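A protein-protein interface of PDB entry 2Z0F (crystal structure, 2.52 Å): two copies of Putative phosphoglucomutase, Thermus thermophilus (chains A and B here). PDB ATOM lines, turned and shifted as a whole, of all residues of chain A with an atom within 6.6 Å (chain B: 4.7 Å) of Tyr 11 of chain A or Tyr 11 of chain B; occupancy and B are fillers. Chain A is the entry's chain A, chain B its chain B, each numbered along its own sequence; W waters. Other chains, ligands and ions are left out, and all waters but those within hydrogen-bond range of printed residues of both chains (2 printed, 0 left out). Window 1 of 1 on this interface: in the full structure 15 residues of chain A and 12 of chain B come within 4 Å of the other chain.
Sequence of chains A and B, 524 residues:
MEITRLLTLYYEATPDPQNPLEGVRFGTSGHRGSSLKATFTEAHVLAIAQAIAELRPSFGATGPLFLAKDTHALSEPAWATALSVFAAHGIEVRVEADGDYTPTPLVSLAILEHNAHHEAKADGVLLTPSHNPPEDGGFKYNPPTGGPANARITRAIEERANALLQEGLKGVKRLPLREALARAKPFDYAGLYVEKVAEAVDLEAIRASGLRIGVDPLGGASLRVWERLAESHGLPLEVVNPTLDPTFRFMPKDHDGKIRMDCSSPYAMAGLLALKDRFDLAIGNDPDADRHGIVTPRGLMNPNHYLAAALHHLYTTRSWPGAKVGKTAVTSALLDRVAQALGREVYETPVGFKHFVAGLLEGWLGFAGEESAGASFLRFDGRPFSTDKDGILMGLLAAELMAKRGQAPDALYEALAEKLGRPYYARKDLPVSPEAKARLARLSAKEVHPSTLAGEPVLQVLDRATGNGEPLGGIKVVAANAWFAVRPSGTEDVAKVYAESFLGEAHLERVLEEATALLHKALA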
ATOM      1  N   LEU A   6      12.790 -13.503  -4.031  1.00  0.00           N
ATOM      2  CA  LEU A   6      11.541 -12.834  -4.376  1.00  0.00           C
ATOM      3  C   LEU A   6      11.781 -11.714  -5.382  1.00  0.00           C
ATOM      4  O   LEU A   6      11.043 -11.579  -6.353  1.00  0.00           O
ATOM      5  CB  LEU A   6      10.880 -12.266  -3.115  1.00  0.00           C
ATOM      6  CG  LEU A   6       9.462 -11.699  -3.257  1.00  0.00           C
ATOM      7  CD1 LEU A   6       8.468 -12.831  -3.435  1.00  0.00           C
ATOM      8  CD2 LEU A   6       9.110 -10.901  -2.025  1.00  0.00           C
ATOM      9  N   LEU A   7      12.813 -10.911  -5.151  1.00  0.00           N
ATOM     10  CA  LEU A   7      13.123  -9.818  -6.065  1.00  0.00           C
ATOM     11  C   LEU A   7      13.764 -10.318  -7.361  1.00  0.00           C
ATOM     12  O   LEU A   7      13.466  -9.809  -8.440  1.00  0.00           O
ATOM     13  CB  LEU A   7      14.034  -8.803  -5.375  1.00  0.00           C
ATOM     14  CG  LEU A   7      13.372  -7.554  -4.772  1.00  0.00           C
ATOM     15  CD1 LEU A   7      12.038  -7.888  -4.149  1.00  0.00           C
ATOM     16  CD2 LEU A   7      14.301  -6.952  -3.735  1.00  0.00           C
ATOM     17  N   THR A   8      14.637 -11.317  -7.266  1.00  0.00           N
ATOM     18  CA  THR A   8      15.279 -11.855  -8.461  1.00  0.00           C
ATOM     19  C   THR A   8      14.192 -12.417  -9.380  1.00  0.00           C
ATOM     20  O   THR A   8      14.229 -12.203 -10.597  1.00  0.00           O
ATOM     21  CB  THR A   8      16.294 -12.985  -8.121  1.00  0.00           C
ATOM     22  OG1 THR A   8      17.337 -12.472  -7.283  1.00  0.00           O
ATOM     23  CG2 THR A   8      16.916 -13.547  -9.387  1.00  0.00           C
ATOM     24  N   LEU A   9      13.220 -13.124  -8.796  1.00  0.00           N
ATOM     25  CA  LEU A   9      12.134 -13.707  -9.582  1.00  0.00           C
ATOM     26  C   LEU A   9      11.230 -12.656 -10.210  1.00  0.00           C
ATOM     27  O   LEU A   9      10.496 -12.937 -11.158  1.00  0.00           O
ATOM     28  CB  LEU A   9      11.303 -14.673  -8.737  1.00  0.00           C
ATOM     29  CG  LEU A   9      12.008 -16.007  -8.460  1.00  0.00           C
ATOM     30  CD1 LEU A   9      11.154 -16.879  -7.559  1.00  0.00           C
ATOM     31  CD2 LEU A   9      12.283 -16.718  -9.770  1.00  0.00           C
ATOM     32  N   TYR A  10      11.283 -11.440  -9.689  1.00  0.00           N
ATOM     33  CA  TYR A  10      10.470 -10.368 -10.242  1.00  0.00           C
ATOM     34  C   TYR A  10      10.936 -10.083 -11.669  1.00  0.00           C
ATOM     35  O   TYR A  10      10.144  -9.752 -12.554  1.00  0.00           O
ATOM     36  CB  TYR A  10      10.630  -9.095  -9.406  1.00  0.00           C
ATOM     37  CG  TYR A  10       9.979  -7.888 -10.037  1.00  0.00           C
ATOM     38  CD1 TYR A  10       8.596  -7.691  -9.953  1.00  0.00           C
ATOM     39  CD2 TYR A  10      10.736  -6.950 -10.743  1.00  0.00           C
ATOM     40  CE1 TYR A  10       7.983  -6.588 -10.557  1.00  0.00           C
ATOM     41  CE2 TYR A  10      10.130  -5.840 -11.356  1.00  0.00           C
ATOM     42  CZ  TYR A  10       8.753  -5.668 -11.255  1.00  0.00           C
ATOM     43  OH  TYR A  10       8.144  -4.579 -11.842  1.00  0.00           O
ATOM     44  N   TYR A  11      12.241 -10.226 -11.874  1.00  0.00           N
ATOM     45  CA  TYR A  11      12.863  -9.953 -13.161  1.00  0.00           C
ATOM     46  C   TYR A  11      13.114 -11.190 -14.011  1.00  0.00           C
ATOM     47  O   TYR A  11      12.983 -11.139 -15.231  1.00  0.00           O
ATOM     48  CB  TYR A  11      14.189  -9.246 -12.926  1.00  0.00           C
ATOM     49  CG  TYR A  11      14.075  -7.863 -12.347  1.00  0.00           C
ATOM     50  CD1 TYR A  11      13.778  -6.771 -13.158  1.00  0.00           C
ATOM     51  CD2 TYR A  11      14.315  -7.634 -10.996  1.00  0.00           C
ATOM     52  CE1 TYR A  11      13.735  -5.483 -12.639  1.00  0.00           C
ATOM     53  CE2 TYR A  11      14.274  -6.346 -10.465  1.00  0.00           C
ATOM     54  CZ  TYR A  11      13.984  -5.280 -11.295  1.00  0.00           C
ATOM     55  OH  TYR A  11      13.942  -4.011 -10.777  1.00  0.00           O
ATOM     56  N   GLU A  12      13.487 -12.297 -13.372  1.00  0.00           N
ATOM     57  CA  GLU A  12      13.767 -13.521 -14.110  1.00  0.00           C
ATOM     58  C   GLU A  12      12.522 -14.292 -14.534  1.00  0.00           C
ATOM     59  O   GLU A  12      12.584 -15.108 -15.454  1.00  0.00           O
ATOM     60  CB  GLU A  12      14.668 -14.453 -13.297  1.00  0.00           C
ATOM     61  CG  GLU A  12      16.047 -13.904 -12.944  1.00  0.00           C
ATOM     62  CD  GLU A  12      16.844 -13.420 -14.146  1.00  0.00           C
ATOM     63  OE1 GLU A  12      16.706 -13.998 -15.248  1.00  0.00           O
ATOM     64  OE2 GLU A  12      17.630 -12.464 -13.976  1.00  0.00           O
ATOM     65  N   ALA A  13      11.396 -14.045 -13.868  1.00  0.00           N
ATOM     66  CA  ALA A  13      10.157 -14.747 -14.203  1.00  0.00           C
ATOM     67  C   ALA A  13       9.218 -13.925 -15.076  1.00  0.00           C
ATOM     68  O   ALA A  13       9.316 -12.700 -15.130  1.00  0.00           O
ATOM     69  CB  ALA A  13       9.434 -15.168 -12.924  1.00  0.00           C
ATOM     70  N   THR A  14       8.317 -14.612 -15.770  1.00  0.00           N
ATOM     71  CA  THR A  14       7.331 -13.960 -16.626  1.00  0.00           C
ATOM     72  C   THR A  14       6.085 -14.823 -16.676  1.00  0.00           C
ATOM     73  O   THR A  14       6.158 -16.035 -16.458  1.00  0.00           O
ATOM     74  CB  THR A  14       7.836 -13.761 -18.088  1.00  0.00           C
ATOM     75  OG1 THR A  14       8.356 -15.000 -18.600  1.00  0.00           O
ATOM     76  CG2 THR A  14       8.899 -12.664 -18.149  1.00  0.00           C
ATOM     77  N   SER A  35       5.878 -12.888  -7.430  1.00  0.00           N
ATOM     78  CA  SER A  35       6.855 -13.317  -8.417  1.00  0.00           C
ATOM     79  C   SER A  35       7.081 -14.812  -8.197  1.00  0.00           C
ATOM     80  O   SER A  35       7.342 -15.559  -9.144  1.00  0.00           O
ATOM     81  CB  SER A  35       8.155 -12.530  -8.246  1.00  0.00           C
ATOM     82  OG  SER A  35       8.620 -12.613  -6.914  1.00  0.00           O
ATOM     83  N   THR A  41       5.238  -9.706 -11.909  1.00  0.00           N
ATOM     84  CA  THR A  41       6.587  -9.573 -12.450  1.00  0.00           C
ATOM     85  C   THR A  41       6.733  -8.300 -13.276  1.00  0.00           C
ATOM     86  O   THR A  41       5.741  -7.667 -13.648  1.00  0.00           O
ATOM     87  CB  THR A  41       6.900 -10.720 -13.398  1.00  0.00           C
ATOM     88  OG1 THR A  41       6.030 -10.625 -14.533  1.00  0.00           O
ATOM     89  CG2 THR A  41       6.687 -12.054 -12.726  1.00  0.00           C
ATOM     90  N   GLU A  42       7.984  -7.961 -13.587  1.00  0.00           N
ATOM     91  CA  GLU A  42       8.306  -6.781 -14.386  1.00  0.00           C
ATOM     92  C   GLU A  42       7.479  -6.741 -15.672  1.00  0.00           C
ATOM     93  O   GLU A  42       7.130  -5.666 -16.166  1.00  0.00           O
ATOM     94  CB  GLU A  42       9.799  -6.776 -14.739  1.00  0.00           C
ATOM     95  CG  GLU A  42      10.218  -5.614 -15.636  1.00  0.00           C
ATOM     96  CD  GLU A  42      11.654  -5.722 -16.131  1.00  0.00           C
ATOM     97  OE1 GLU A  42      11.979  -6.717 -16.817  1.00  0.00           O
ATOM     98  OE2 GLU A  42      12.456  -4.810 -15.837  1.00  0.00           O
ATOM     99  N   GLU A  76       9.303  -1.983  -4.523  1.00  0.00           N
ATOM    100  CA  GLU A  76      10.529  -1.289  -4.903  1.00  0.00           C
ATOM    101  C   GLU A  76      10.755  -1.381  -6.421  1.00  0.00           C
ATOM    102  O   GLU A  76      10.670  -0.381  -7.133  1.00  0.00           O
ATOM    103  CB  GLU A  76      11.711  -1.913  -4.161  1.00  0.00           C
ATOM    104  CG  GLU A  76      12.989  -1.138  -4.256  1.00  0.00           C
ATOM    105  CD  GLU A  76      13.067  -0.053  -3.216  1.00  0.00           C
ATOM    106  OE1 GLU A  76      12.248   0.889  -3.269  1.00  0.00           O
ATOM    107  OE2 GLU A  76      13.950  -0.152  -2.336  1.00  0.00           O
ATOM    108  N   PRO A  77      11.028  -2.589  -6.940  1.00  0.00           N
ATOM    109  CA  PRO A  77      11.247  -2.690  -8.385  1.00  0.00           C
ATOM    110  C   PRO A  77      10.061  -2.228  -9.231  1.00  0.00           C
ATOM    111  O   PRO A  77      10.244  -1.703 -10.335  1.00  0.00           O
ATOM    112  CB  PRO A  77      11.567  -4.172  -8.581  1.00  0.00           C
ATOM    113  CG  PRO A  77      10.794  -4.834  -7.495  1.00  0.00           C
ATOM    114  CD  PRO A  77      11.044  -3.925  -6.313  1.00  0.00           C
ATOM    115  N   ALA A  78       8.847  -2.422  -8.721  1.00  0.00           N
ATOM    116  CA  ALA A  78       7.648  -2.018  -9.455  1.00  0.00           C
ATOM    117  C   ALA A  78       7.643  -0.507  -9.624  1.00  0.00           C
ATOM    118  O   ALA A  78       7.241   0.014 -10.654  1.00  0.00           O
ATOM    119  CB  ALA A  78       6.407  -2.475  -8.712  1.00  0.00           C
ATOM    120  N   ALA A  80      10.312   1.367  -9.781  1.00  0.00           N
ATOM    121  CA  ALA A  80      11.340   1.607 -10.785  1.00  0.00           C
ATOM    122  C   ALA A  80      10.790   1.364 -12.189  1.00  0.00           C
ATOM    123  O   ALA A  80      10.934   2.211 -13.082  1.00  0.00           O
ATOM    124  CB  ALA A  80      12.531   0.700 -10.523  1.00  0.00           C
ATOM    125  N   THR A  81      10.149   0.216 -12.383  1.00  0.00           N
ATOM    126  CA  THR A  81       9.578  -0.124 -13.683  1.00  0.00           C
ATOM    127  C   THR A  81       8.515   0.873 -14.152  1.00  0.00           C
ATOM    128  O   THR A  81       8.544   1.349 -15.291  1.00  0.00           O
ATOM    129  CB  THR A  81       8.932  -1.516 -13.654  1.00  0.00           C
ATOM    130  OG1 THR A  81       9.912  -2.490 -13.276  1.00  0.00           O
ATOM    131  CG2 THR A  81       8.372  -1.865 -15.015  1.00  0.00           C
ATOM    132  N   ARG A 174      10.197   2.764 -22.673  1.00  0.00           N
ATOM    133  CA  ARG A 174      10.621   3.170 -21.339  1.00  0.00           C
ATOM    134  C   ARG A 174      11.968   3.867 -21.395  1.00  0.00           C
ATOM    135  O   ARG A 174      12.556   4.030 -22.463  1.00  0.00           O
ATOM    136  CB  ARG A 174      10.753   1.944 -20.443  1.00  0.00           C
ATOM    137  CG  ARG A 174      11.733   0.928 -21.004  1.00  0.00           C
ATOM    138  CD  ARG A 174      11.984  -0.170 -20.021  1.00  0.00           C
ATOM    139  NE  ARG A 174      12.581   0.349 -18.799  1.00  0.00           N
ATOM    140  CZ  ARG A 174      12.785  -0.376 -17.704  1.00  0.00           C
ATOM    141  NH1 ARG A 174      12.434  -1.656 -17.682  1.00  0.00           N
ATOM    142  NH2 ARG A 174      13.334   0.182 -16.632  1.00  0.00           N
ATOM    143  N   LEU B   7      19.124  -5.037  -4.979  1.00  0.00           N
ATOM    144  CA  LEU B   7      18.824  -5.968  -6.061  1.00  0.00           C
ATOM    145  C   LEU B   7      18.132  -5.287  -7.225  1.00  0.00           C
ATOM    146  O   LEU B   7      18.297  -5.693  -8.376  1.00  0.00           O
ATOM    147  CB  LEU B   7      17.975  -7.142  -5.568  1.00  0.00           C
ATOM    148  CG  LEU B   7      18.833  -8.264  -4.985  1.00  0.00           C
ATOM    149  CD1 LEU B   7      19.172  -7.956  -3.545  1.00  0.00           C
ATOM    150  CD2 LEU B   7      18.099  -9.572  -5.079  1.00  0.00           C
ATOM    151  N   THR B   8      17.365  -4.242  -6.936  1.00  0.00           N
ATOM    152  CA  THR B   8      16.668  -3.528  -7.996  1.00  0.00           C
ATOM    153  C   THR B   8      17.719  -2.824  -8.849  1.00  0.00           C
ATOM    154  O   THR B   8      17.591  -2.740 -10.071  1.00  0.00           O
ATOM    155  CB  THR B   8      15.657  -2.473  -7.424  1.00  0.00           C
ATOM    156  OG1 THR B   8      14.721  -3.113  -6.539  1.00  0.00           O
ATOM    157  CG2 THR B   8      14.878  -1.823  -8.545  1.00  0.00           C
ATOM    158  N   LEU B   9      18.770  -2.326  -8.211  1.00  0.00           N
ATOM    159  CA  LEU B   9      19.798  -1.642  -8.970  1.00  0.00           C
ATOM    160  C   LEU B   9      20.613  -2.611  -9.830  1.00  0.00           C
ATOM    161  O   LEU B   9      21.041  -2.250 -10.931  1.00  0.00           O
ATOM    162  CB  LEU B   9      20.699  -0.825  -8.044  1.00  0.00           C
ATOM    163  CG  LEU B   9      19.993   0.433  -7.504  1.00  0.00           C
ATOM    164  CD1 LEU B   9      20.981   1.313  -6.735  1.00  0.00           C
ATOM    165  CD2 LEU B   9      19.392   1.211  -8.661  1.00  0.00           C
ATOM    166  N   TYR B  10      20.808  -3.837  -9.343  1.00  0.00           N
ATOM    167  CA  TYR B  10      21.543  -4.841 -10.111  1.00  0.00           C
ATOM    168  C   TYR B  10      20.936  -4.920 -11.518  1.00  0.00           C
ATOM    169  O   TYR B  10      21.649  -4.922 -12.527  1.00  0.00           O
ATOM    170  CB  TYR B  10      21.442  -6.211  -9.438  1.00  0.00           C
ATOM    171  CG  TYR B  10      21.977  -7.355 -10.284  1.00  0.00           C
ATOM    172  CD1 TYR B  10      23.313  -7.741 -10.209  1.00  0.00           C
ATOM    173  CD2 TYR B  10      21.140  -8.056 -11.158  1.00  0.00           C
ATOM    174  CE1 TYR B  10      23.805  -8.801 -10.979  1.00  0.00           C
ATOM    175  CE2 TYR B  10      21.620  -9.113 -11.929  1.00  0.00           C
ATOM    176  CZ  TYR B  10      22.954  -9.483 -11.834  1.00  0.00           C
ATOM    177  OH  TYR B  10      23.431 -10.538 -12.585  1.00  0.00           O
ATOM    178  N   TYR B  11      19.609  -4.965 -11.566  1.00  0.00           N
ATOM    179  CA  TYR B  11      18.874  -5.042 -12.820  1.00  0.00           C
ATOM    180  C   TYR B  11      18.608  -3.683 -13.455  1.00  0.00           C
ATOM    181  O   TYR B  11      18.651  -3.538 -14.673  1.00  0.00           O
ATOM    182  CB  TYR B  11      17.530  -5.732 -12.589  1.00  0.00           C
ATOM    183  CG  TYR B  11      17.618  -7.210 -12.305  1.00  0.00           C
ATOM    184  CD1 TYR B  11      17.786  -8.132 -13.339  1.00  0.00           C
ATOM    185  CD2 TYR B  11      17.519  -7.690 -11.007  1.00  0.00           C
ATOM    186  CE1 TYR B  11      17.852  -9.500 -13.082  1.00  0.00           C
ATOM    187  CE2 TYR B  11      17.580  -9.054 -10.735  1.00  0.00           C
ATOM    188  CZ  TYR B  11      17.750  -9.956 -11.776  1.00  0.00           C
ATOM    189  OH  TYR B  11      17.841 -11.309 -11.497  1.00  0.00           O
ATOM    190  N   GLU B  12      18.336  -2.681 -12.633  1.00  0.00           N
ATOM    191  CA  GLU B  12      17.999  -1.366 -13.155  1.00  0.00           C
ATOM    192  C   GLU B  12      19.187  -0.478 -13.532  1.00  0.00           C
ATOM    193  O   GLU B  12      19.061   0.409 -14.376  1.00  0.00           O
ATOM    194  CB  GLU B  12      17.100  -0.654 -12.143  1.00  0.00           C
ATOM    195  CG  GLU B  12      15.865   0.020 -12.742  1.00  0.00           C
ATOM    196  CD  GLU B  12      14.883  -0.950 -13.388  1.00  0.00           C
ATOM    197  OE1 GLU B  12      14.366  -1.859 -12.700  1.00  0.00           O
ATOM    198  OE2 GLU B  12      14.620  -0.786 -14.596  1.00  0.00           O
ATOM    199  N   ALA B  13      20.339  -0.716 -12.915  1.00  0.00           N
ATOM    200  CA  ALA B  13      21.529   0.082 -13.200  1.00  0.00           C
ATOM    201  C   ALA B  13      22.462  -0.569 -14.225  1.00  0.00           C
ATOM    202  O   ALA B  13      22.613  -1.789 -14.250  1.00  0.00           O
ATOM    203  CB  ALA B  13      22.290   0.343 -11.910  1.00  0.00           C
ATOM    204  N   GLU B  42      23.559  -6.518 -13.813  1.00  0.00           N
ATOM    205  CA  GLU B  42      23.209  -7.632 -14.678  1.00  0.00           C
ATOM    206  C   GLU B  42      24.059  -7.513 -15.939  1.00  0.00           C
ATOM    207  O   GLU B  42      24.444  -8.514 -16.540  1.00  0.00           O
ATOM    208  CB  GLU B  42      21.725  -7.563 -15.059  1.00  0.00           C
ATOM    209  CG  GLU B  42      21.145  -8.869 -15.576  1.00  0.00           C
ATOM    210  CD  GLU B  42      19.915  -8.667 -16.427  1.00  0.00           C
ATOM    211  OE1 GLU B  42      19.124  -9.624 -16.578  1.00  0.00           O
ATOM    212  OE2 GLU B  42      19.741  -7.553 -16.962  1.00  0.00           O
ATOM    213  N   PRO B  77      21.078 -12.828  -7.789  1.00  0.00           N
ATOM    214  CA  PRO B  77      20.763 -12.475  -9.174  1.00  0.00           C
ATOM    215  C   PRO B  77      21.861 -12.919 -10.148  1.00  0.00           C
ATOM    216  O   PRO B  77      21.569 -13.392 -11.250  1.00  0.00           O
ATOM    217  CB  PRO B  77      20.625 -10.950  -9.131  1.00  0.00           C
ATOM    218  CG  PRO B  77      20.411 -10.630  -7.681  1.00  0.00           C
ATOM    219  CD  PRO B  77      21.267 -11.619  -6.971  1.00  0.00           C
HETATM  220  O   HOH W   1      12.248  -2.414 -15.040  1.00  0.00           O
HETATM  221  O   HOH W   2      19.650 -11.729 -15.312  1.00  0.00           O
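Tyr 11 of chain A touches just these residues of chain B: Thr 8 (3.3 Å), Tyr 11 (3.2 Å) and Glu 12 (2.9 Å). Of chain A, only Thr 8, Tyr 11 and Glu 12 come within 4 Å of Tyr 11 of chain B. Of the printed residues of chain B, Glu 76 of chain A touches Thr 8 (3.5 Å). Printed residues of chain B within 4 Å of Arg 174 of chain A: Glu 12 (2.6 Å). Of the printed residues of chain B, Ala 80 of chain A touches Thr 8 (3.97 Å) and Glu 12 (3.8 Å). Printed residues of chain A within 4 Å of Pro 77 of chain B: Thr 8 (3.6 Å). Thr 81 of chain A touches none of the printed residues of chain B. Thr 41 of chain A touches none of the printed residues of chain B. The nearest residue of chain A that does not touch Tyr 11 of chain B is Leu 7 of chain A (4.8 Å).
Among the printed residues, pairs that only touch across the chains: Tyr 11 of chain A with Tyr 11 of chain B (3.2 Å), Thr 8 of chain A with Tyr 11 of chain B (3.2 Å), Tyr 11 of chain A with Thr 8 of chain B (3.3 Å), Glu 76 of chain A with Thr 8 of chain B (3.5 Å), Thr 8 of chain A with Pro 77 of chain B (3.6 Å), Thr 8 of chain A with Leu 7 of chain B (3.7 Å), Pro 77 of chain A with Thr 8 of chain B (3.7 Å), Ala 80 of chain A with Glu 12 of chain B (3.8 Å) and Ala 80 of chain A with Thr 8 of chain B (3.97 Å).
Of the 18 printed residues of chain A, 7 touch a printed residue of chain B. Hydrophobic or aromatic side chains of chain A within 4 Å of the printed part of chain B: Tyr 11, Pro 77 and Ala 80. Among the printed residues, 12 pairs touch across the chains. Among the printed residues, Asp or Glu carboxylates within 4 Å of a Lys or Arg side-chain nitrogen of the other chain: Arg 174 of chain A with Glu 12 of chain B (2.6 Å).
Thr 8 of chain A touches Leu 7 of chain B, but with the chains exchanged Leu 7 of chain A does not touch Thr 8 of chain B (4.8 Å). Thr 8 of chain A touches Pro 77 of chain B, and with the chains exchanged Pro 77 of chain A touches Thr 8 of chain B. Tyr 11 of chain B touches its own counterpart, Tyr 11 of chain A. Tyr 11 of chain A touches Glu 12 of chain B, and with the chains exchanged Glu 12 of chain A touches Tyr 11 of chain B. Of the 12 pairs that touch across the chains among the printed residues, 7 have their exchanged pair printed and touching as well.
OH of Tyr 11 of chain A lies within hydrogen-bond range of OE1 of Glu 12 of chain B, at 2.9 Å. The side-chain carboxylate of Glu 12 of chain A sits at hydrogen-bond distance from the side-chain hydroxyl of Tyr 11 of chain B, at 2.7 Å. The side-chain carboxylate (OE2) of Glu 12 of chain B lies within salt-bridge range of the guanidinium group (NH2) of Arg 174 of chain A.
Water W2 bridges the side-chain carboxylate of Glu 42 of chain B (2.5 Å) and the side-chain carboxylate of Glu 12 of chain A (2.5 Å). Water W1 lies within hydrogen-bond range of OE2 of Glu 42 of chain A (2.5 Å), NH1 of Arg 174 of chain A (2.8 Å), OE2 of Glu 12 of chain B (2.9 Å) and OG1 of Thr 81 of chain A (2.9 Å).
NH1 of Arg 174 of chain A lies within salt-bridge range of OE2 of Glu 42 of chain A (3.7 Å). The backbone carbonyl oxygen of Pro 77 of chain A is in hydrogen-bond range of the side-chain hydroxyl of Thr 81 of chain A, at 3.1 Å.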
